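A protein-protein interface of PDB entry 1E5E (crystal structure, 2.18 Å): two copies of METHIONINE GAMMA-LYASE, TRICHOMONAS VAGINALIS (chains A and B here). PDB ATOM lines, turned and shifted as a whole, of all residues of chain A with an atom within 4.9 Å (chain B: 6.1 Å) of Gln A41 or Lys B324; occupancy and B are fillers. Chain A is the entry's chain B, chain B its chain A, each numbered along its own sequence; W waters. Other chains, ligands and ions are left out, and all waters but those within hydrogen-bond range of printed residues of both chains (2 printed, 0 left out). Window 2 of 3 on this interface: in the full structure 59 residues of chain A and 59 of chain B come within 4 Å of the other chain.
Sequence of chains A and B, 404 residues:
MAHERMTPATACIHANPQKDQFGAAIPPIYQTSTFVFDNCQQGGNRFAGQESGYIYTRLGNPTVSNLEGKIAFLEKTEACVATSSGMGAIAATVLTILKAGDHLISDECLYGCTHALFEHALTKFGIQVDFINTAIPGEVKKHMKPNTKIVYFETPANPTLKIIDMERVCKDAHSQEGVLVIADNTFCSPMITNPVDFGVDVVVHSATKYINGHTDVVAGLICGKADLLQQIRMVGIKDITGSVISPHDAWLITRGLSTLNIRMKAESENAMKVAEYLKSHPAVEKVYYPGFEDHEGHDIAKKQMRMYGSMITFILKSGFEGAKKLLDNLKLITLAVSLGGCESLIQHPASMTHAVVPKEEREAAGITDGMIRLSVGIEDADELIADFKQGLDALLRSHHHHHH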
ATOM      1  N   ASN A  39      -6.365 -20.238  -4.039  1.00  0.00           N
ATOM      2  CA  ASN A  39      -5.988 -18.992  -4.686  1.00  0.00           C
ATOM      3  C   ASN A  39      -6.994 -18.686  -5.770  1.00  0.00           C
ATOM      4  O   ASN A  39      -7.801 -19.584  -6.092  1.00  0.00           O
ATOM      5  CB  ASN A  39      -4.553 -19.023  -5.210  1.00  0.00           C
ATOM      6  CG  ASN A  39      -4.354 -20.207  -6.126  1.00  0.00           C
ATOM      7  OD1 ASN A  39      -4.914 -20.285  -7.211  1.00  0.00           O
ATOM      8  ND2 ASN A  39      -3.606 -21.183  -5.682  1.00  0.00           N
ATOM      9  N   CYS A  40      -6.967 -17.469  -6.306  1.00  0.00           N
ATOM     10  CA  CYS A  40      -7.947 -17.116  -7.345  1.00  0.00           C
ATOM     11  C   CYS A  40      -7.856 -17.933  -8.611  1.00  0.00           C
ATOM     12  O   CYS A  40      -8.876 -18.209  -9.248  1.00  0.00           O
ATOM     13  CB  CYS A  40      -7.820 -15.654  -7.811  1.00  0.00           C
ATOM     14  SG  CYS A  40      -8.248 -14.510  -6.511  1.00  0.00           S
ATOM     15  N   GLN A  41      -6.626 -18.244  -8.983  1.00  0.00           N
ATOM     16  CA  GLN A  41      -6.432 -19.027 -10.213  1.00  0.00           C
ATOM     17  C   GLN A  41      -7.129 -20.384 -10.101  1.00  0.00           C
ATOM     18  O   GLN A  41      -7.789 -20.855 -11.030  1.00  0.00           O
ATOM     19  CB  GLN A  41      -4.932 -19.206 -10.481  1.00  0.00           C
ATOM     20  CG  GLN A  41      -4.652 -20.032 -11.735  1.00  0.00           C
ATOM     21  CD  GLN A  41      -4.797 -19.136 -12.951  1.00  0.00           C
ATOM     22  OE1 GLN A  41      -4.238 -18.037 -12.929  1.00  0.00           O
ATOM     23  NE2 GLN A  41      -5.516 -19.586 -13.961  1.00  0.00           N
ATOM     24  N   GLN A  42      -6.979 -21.041  -8.964  1.00  0.00           N
ATOM     25  CA  GLN A  42      -7.630 -22.344  -8.727  1.00  0.00           C
ATOM     26  C   GLN A  42      -9.138 -22.207  -8.828  1.00  0.00           C
ATOM     27  O   GLN A  42      -9.852 -22.972  -9.487  1.00  0.00           O
ATOM     28  CB  GLN A  42      -7.163 -22.855  -7.344  1.00  0.00           C
ATOM     29  CG  GLN A  42      -7.828 -24.149  -6.916  1.00  0.00           C
ATOM     30  CD  GLN A  42      -7.614 -24.546  -5.470  1.00  0.00           C
ATOM     31  OE1 GLN A  42      -8.334 -24.097  -4.575  1.00  0.00           O
ATOM     32  NE2 GLN A  42      -6.620 -25.395  -5.231  1.00  0.00           N
ATOM     33  N   GLY A  43      -9.698 -21.178  -8.203  1.00  0.00           N
ATOM     34  CA  GLY A  43     -11.137 -20.897  -8.258  1.00  0.00           C
ATOM     35  C   GLY A  43     -11.607 -20.719  -9.697  1.00  0.00           C
ATOM     36  O   GLY A  43     -12.580 -21.325 -10.153  1.00  0.00           O
ATOM     37  N   GLY A  44     -10.913 -19.857 -10.474  1.00  0.00           N
ATOM     38  CA  GLY A  44     -11.293 -19.656 -11.873  1.00  0.00           C
ATOM     39  C   GLY A  44     -11.105 -20.944 -12.685  1.00  0.00           C
ATOM     40  O   GLY A  44     -11.973 -21.219 -13.538  1.00  0.00           O
ATOM     41  N   ASN A  45     -10.101 -21.767 -12.374  1.00  0.00           N
ATOM     42  CA  ASN A  45      -9.929 -23.013 -13.124  1.00  0.00           C
ATOM     43  C   ASN A  45     -11.078 -23.988 -12.864  1.00  0.00           C
ATOM     44  O   ASN A  45     -11.591 -24.595 -13.794  1.00  0.00           O
ATOM     45  CB  ASN A  45      -8.600 -23.709 -12.825  1.00  0.00           C
ATOM     46  CG  ASN A  45      -7.402 -22.986 -13.443  1.00  0.00           C
ATOM     47  OD1 ASN A  45      -7.590 -22.209 -14.374  1.00  0.00           O
ATOM     48  ND2 ASN A  45      -6.187 -23.173 -12.945  1.00  0.00           N
ATOM     49  N   GLU A  51     -10.131 -27.629 -13.769  1.00  0.00           N
ATOM     50  CA  GLU A  51      -9.418 -28.205 -12.623  1.00  0.00           C
ATOM     51  C   GLU A  51     -10.420 -28.905 -11.718  1.00  0.00           C
ATOM     52  O   GLU A  51     -11.584 -28.510 -11.679  1.00  0.00           O
ATOM     53  CB  GLU A  51      -8.646 -27.146 -11.864  1.00  0.00           C
ATOM     54  CG  GLU A  51      -7.740 -27.669 -10.779  1.00  0.00           C
ATOM     55  CD  GLU A  51      -6.827 -26.606 -10.183  1.00  0.00           C
ATOM     56  OE1 GLU A  51      -6.651 -25.527 -10.779  1.00  0.00           O
ATOM     57  OE2 GLU A  51      -6.277 -26.871  -9.098  1.00  0.00           O
ATOM     58  N   LEU B 316     -10.378  -2.402  -7.856  1.00  0.00           N
ATOM     59  CA  LEU B 316      -9.026  -1.940  -7.623  1.00  0.00           C
ATOM     60  C   LEU B 316      -8.511  -1.226  -8.892  1.00  0.00           C
ATOM     61  O   LEU B 316      -8.763  -1.655 -10.015  1.00  0.00           O
ATOM     62  CB  LEU B 316      -8.029  -3.029  -7.278  1.00  0.00           C
ATOM     63  CG  LEU B 316      -8.299  -3.858  -6.015  1.00  0.00           C
ATOM     64  CD1 LEU B 316      -7.332  -5.046  -5.937  1.00  0.00           C
ATOM     65  CD2 LEU B 316      -8.272  -3.030  -4.753  1.00  0.00           C
ATOM     66  N   GLY B 319      -6.768  -3.304 -11.540  1.00  0.00           N
ATOM     67  CA  GLY B 319      -7.477  -4.287 -12.319  1.00  0.00           C
ATOM     68  C   GLY B 319      -7.415  -5.738 -11.862  1.00  0.00           C
ATOM     69  O   GLY B 319      -7.379  -6.072 -10.681  1.00  0.00           O
ATOM     70  N   PHE B 320      -7.478  -6.625 -12.846  1.00  0.00           N
ATOM     71  CA  PHE B 320      -7.572  -8.058 -12.672  1.00  0.00           C
ATOM     72  C   PHE B 320      -6.424  -8.662 -11.885  1.00  0.00           C
ATOM     73  O   PHE B 320      -6.613  -9.341 -10.872  1.00  0.00           O
ATOM     74  CB  PHE B 320      -7.703  -8.732 -14.039  1.00  0.00           C
ATOM     75  CG  PHE B 320      -7.785 -10.234 -14.016  1.00  0.00           C
ATOM     76  CD1 PHE B 320      -8.734 -10.906 -13.271  1.00  0.00           C
ATOM     77  CD2 PHE B 320      -6.839 -10.989 -14.701  1.00  0.00           C
ATOM     78  CE1 PHE B 320      -8.769 -12.291 -13.220  1.00  0.00           C
ATOM     79  CE2 PHE B 320      -6.889 -12.376 -14.689  1.00  0.00           C
ATOM     80  CZ  PHE B 320      -7.864 -13.034 -13.957  1.00  0.00           C
ATOM     81  N   GLU B 321      -5.202  -8.291 -12.286  1.00  0.00           N
ATOM     82  CA  GLU B 321      -3.999  -8.812 -11.650  1.00  0.00           C
ATOM     83  C   GLU B 321      -3.937  -8.312 -10.216  1.00  0.00           C
ATOM     84  O   GLU B 321      -3.510  -9.048  -9.329  1.00  0.00           O
ATOM     85  CB  GLU B 321      -2.730  -8.457 -12.443  1.00  0.00           C
ATOM     86  CG  GLU B 321      -2.714  -9.167 -13.792  1.00  0.00           C
ATOM     87  CD  GLU B 321      -2.478 -10.659 -13.678  1.00  0.00           C
ATOM     88  OE1 GLU B 321      -1.767 -11.158 -12.780  1.00  0.00           O
ATOM     89  OE2 GLU B 321      -2.979 -11.443 -14.510  1.00  0.00           O
ATOM     90  N   GLY B 322      -4.317  -7.047  -9.999  1.00  0.00           N
ATOM     91  CA  GLY B 322      -4.352  -6.539  -8.631  1.00  0.00           C
ATOM     92  C   GLY B 322      -5.401  -7.305  -7.814  1.00  0.00           C
ATOM     93  O   GLY B 322      -5.153  -7.558  -6.627  1.00  0.00           O
ATOM     94  N   ALA B 323      -6.579  -7.610  -8.355  1.00  0.00           N
ATOM     95  CA  ALA B 323      -7.588  -8.337  -7.600  1.00  0.00           C
ATOM     96  C   ALA B 323      -7.055  -9.700  -7.140  1.00  0.00           C
ATOM     97  O   ALA B 323      -7.298 -10.140  -6.001  1.00  0.00           O
ATOM     98  CB  ALA B 323      -8.843  -8.507  -8.463  1.00  0.00           C
ATOM     99  N   LYS B 324      -6.399 -10.448  -8.017  1.00  0.00           N
ATOM    100  CA  LYS B 324      -5.855 -11.747  -7.651  1.00  0.00           C
ATOM    101  C   LYS B 324      -4.821 -11.649  -6.540  1.00  0.00           C
ATOM    102  O   LYS B 324      -4.857 -12.425  -5.575  1.00  0.00           O
ATOM    103  CB  LYS B 324      -5.265 -12.430  -8.881  1.00  0.00           C
ATOM    104  CG  LYS B 324      -6.374 -12.790  -9.878  1.00  0.00           C
ATOM    105  CD  LYS B 324      -5.897 -13.873 -10.832  1.00  0.00           C
ATOM    106  CE  LYS B 324      -4.941 -13.282 -11.880  1.00  0.00           C
ATOM    107  NZ  LYS B 324      -4.123 -14.344 -12.558  1.00  0.00           N
ATOM    108  N   LYS B 325      -3.918 -10.680  -6.643  1.00  0.00           N
ATOM    109  CA  LYS B 325      -2.907 -10.540  -5.605  1.00  0.00           C
ATOM    110  C   LYS B 325      -3.560 -10.244  -4.257  1.00  0.00           C
ATOM    111  O   LYS B 325      -3.037 -10.657  -3.222  1.00  0.00           O
ATOM    112  CB  LYS B 325      -1.845  -9.491  -5.894  1.00  0.00           C
ATOM    113  N   LEU B 326      -4.536  -9.341  -4.243  1.00  0.00           N
ATOM    114  CA  LEU B 326      -5.161  -9.017  -2.958  1.00  0.00           C
ATOM    115  C   LEU B 326      -5.893 -10.236  -2.394  1.00  0.00           C
ATOM    116  O   LEU B 326      -5.720 -10.539  -1.234  1.00  0.00           O
ATOM    117  CB  LEU B 326      -6.172  -7.876  -3.104  1.00  0.00           C
ATOM    118  CG  LEU B 326      -7.046  -7.589  -1.871  1.00  0.00           C
ATOM    119  CD1 LEU B 326      -6.213  -7.001  -0.746  1.00  0.00           C
ATOM    120  CD2 LEU B 326      -8.204  -6.677  -2.272  1.00  0.00           C
ATOM    121  N   LEU B 327      -6.686 -10.931  -3.222  1.00  0.00           N
ATOM    122  CA  LEU B 327      -7.478 -12.062  -2.771  1.00  0.00           C
ATOM    123  C   LEU B 327      -6.605 -13.243  -2.351  1.00  0.00           C
ATOM    124  O   LEU B 327      -6.894 -13.734  -1.266  1.00  0.00           O
ATOM    125  CB  LEU B 327      -8.560 -12.494  -3.744  1.00  0.00           C
ATOM    126  CG  LEU B 327      -9.914 -11.750  -3.603  1.00  0.00           C
ATOM    127  CD1 LEU B 327      -9.784 -10.252  -3.366  1.00  0.00           C
ATOM    128  CD2 LEU B 327     -10.711 -12.030  -4.870  1.00  0.00           C
ATOM    129  N   ASP B 328      -5.449 -13.384  -3.011  1.00  0.00           N
ATOM    130  CA  ASP B 328      -4.551 -14.434  -2.574  1.00  0.00           C
ATOM    131  C   ASP B 328      -3.809 -14.054  -1.310  1.00  0.00           C
ATOM    132  O   ASP B 328      -3.234 -14.994  -0.772  1.00  0.00           O
ATOM    133  CB  ASP B 328      -3.510 -14.778  -3.661  1.00  0.00           C
ATOM    134  CG  ASP B 328      -4.228 -15.345  -4.871  1.00  0.00           C
ATOM    135  OD1 ASP B 328      -5.451 -15.612  -4.855  1.00  0.00           O
ATOM    136  OD2 ASP B 328      -3.584 -15.525  -5.930  1.00  0.00           O
ATOM    137  N   ASN B 329      -3.753 -12.824  -0.828  1.00  0.00           N
ATOM    138  CA  ASN B 329      -2.946 -12.558   0.370  1.00  0.00           C
ATOM    139  C   ASN B 329      -3.743 -12.217   1.624  1.00  0.00           C
ATOM    140  O   ASN B 329      -3.261 -11.726   2.651  1.00  0.00           O
ATOM    141  CB  ASN B 329      -1.957 -11.442  -0.034  1.00  0.00           C
ATOM    142  CG  ASN B 329      -0.893 -12.009  -0.971  1.00  0.00           C
ATOM    143  OD1 ASN B 329      -0.147 -12.933  -0.594  1.00  0.00           O
ATOM    144  ND2 ASN B 329      -0.905 -11.625  -2.242  1.00  0.00           N
ATOM    145  N   HIS B 348     -14.252 -13.089  -6.907  1.00  0.00           N
ATOM    146  CA  HIS B 348     -14.004 -12.264  -8.092  1.00  0.00           C
ATOM    147  C   HIS B 348     -15.049 -12.626  -9.128  1.00  0.00           C
ATOM    148  O   HIS B 348     -14.915 -13.672  -9.772  1.00  0.00           O
ATOM    149  CB  HIS B 348     -12.567 -12.579  -8.566  1.00  0.00           C
ATOM    150  CG  HIS B 348     -12.251 -11.878  -9.860  1.00  0.00           C
ATOM    151  ND1 HIS B 348     -12.369 -12.482 -11.097  1.00  0.00           N
ATOM    152  CD2 HIS B 348     -11.909 -10.579 -10.098  1.00  0.00           C
ATOM    153  CE1 HIS B 348     -12.052 -11.614 -12.043  1.00  0.00           C
ATOM    154  NE2 HIS B 348     -11.756 -10.458 -11.457  1.00  0.00           N
ATOM    155  N   MET B 352     -15.514 -16.055 -11.453  1.00  0.00           N
ATOM    156  CA  MET B 352     -16.129 -17.004 -10.527  1.00  0.00           C
ATOM    157  C   MET B 352     -17.636 -17.031 -10.621  1.00  0.00           C
ATOM    158  O   MET B 352     -18.172 -17.651 -11.567  1.00  0.00           O
ATOM    159  CB  MET B 352     -15.674 -16.718  -9.072  1.00  0.00           C
ATOM    160  CG  MET B 352     -14.146 -16.874  -8.965  1.00  0.00           C
ATOM    161  SD  MET B 352     -13.568 -16.482  -7.312  1.00  0.00           S
ATOM    162  CE  MET B 352     -11.802 -16.506  -7.563  1.00  0.00           C
ATOM    163  N   ILE B 372     -14.322  -6.830  -7.297  1.00  0.00           N
ATOM    164  CA  ILE B 372     -14.274  -7.778  -6.196  1.00  0.00           C
ATOM    165  C   ILE B 372     -15.575  -7.700  -5.393  1.00  0.00           C
ATOM    166  O   ILE B 372     -16.024  -6.570  -5.123  1.00  0.00           O
ATOM    167  CB  ILE B 372     -13.092  -7.429  -5.266  1.00  0.00           C
ATOM    168  CG1 ILE B 372     -11.796  -7.651  -6.036  1.00  0.00           C
ATOM    169  CG2 ILE B 372     -13.086  -8.294  -4.000  1.00  0.00           C
ATOM    170  CD1 ILE B 372     -10.543  -7.024  -5.473  1.00  0.00           C
HETATM  171  O   HOH W   1      -5.879 -16.225 -13.904  1.00  0.00           O
HETATM  172  O   HOH W   2      -4.374 -16.769  -8.060  1.00  0.00           O
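Of the 8 printed residues of chain A, 3 touch a printed residue of chain B. Among the printed residues, no Asp or Glu carboxylate lies within 4 Å of a Lys or Arg side-chain nitrogen of the other chain.
The side-chain carboxylate (OD1) of Asp B328 sits at hydrogen-bond distance from the backbone NH (N) of Cys A40.
Printed residues of chain B within 4 Å of Gln A41: Lys B324 (3.7 Å). Of the printed residues of chain A, Lys B324 touches Cys A40 (3.8 Å) and Gln A41 (3.7 Å). Printed residues of chain A within 4 Å of Asp B328: Asn A39 (3.4 Å) and Cys A40 (2.8 Å). Of the printed residues of chain B, Asn A39 touches Asp B328 (3.4 Å). Ala B323 touches none of the printed residues of chain A. Leu B326 touches none of the printed residues of chain A. The nearest printed residue of chain B that does not touch Gln A41 is Asp B328 (5.0 Å). The nearest printed residue of chain A that does not touch Lys B324 is Asn A39 (6.6 Å). The nearest printed residue of chain B that does not touch Asn A39 is Met B352 (5.3 Å).
Water W2 lies within hydrogen-bond range of the side-chain carboxylate of Asp B328, the backbone NH of Gln A41 and the backbone NH of Cys A40. Water W1 lies within hydrogen-bond range of the side-chain amide oxygen of Gln A41 and the side-chain amino group of Lys B324.
No position is printed for both chains. Of the 6 pairs that touch across the chains among the printed residues, none has its exchanged pair printed and touching as well.
N of His B348 sits at hydrogen-bond distance from SD of Met B352 (3.5 Å). The side-chain amide oxygen (OD1) of Asn A39 lies within hydrogen-bond range of the backbone NH (N) of Gln A42 (2.8 Å). The side-chain amide oxygen (OD1) of Asn A39 lies within hydrogen-bond range of the backbone NH (N) of Gln A41, at 3.2 Å. OD1 of Asn A45 is in hydrogen-bond range of NE2 of Gln A41 (3.4 Å). OE2 of Glu B321 is in salt-bridge range of NZ of Lys B324 (3.7 Å).
Among the printed residues, pairs that only touch across the chains: Asn A39 with Asp B328, Cys A40 with Lys B324, Cys A40 with Leu B327, Cys A40 with Met B352 and Gln A41 with Lys B324.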
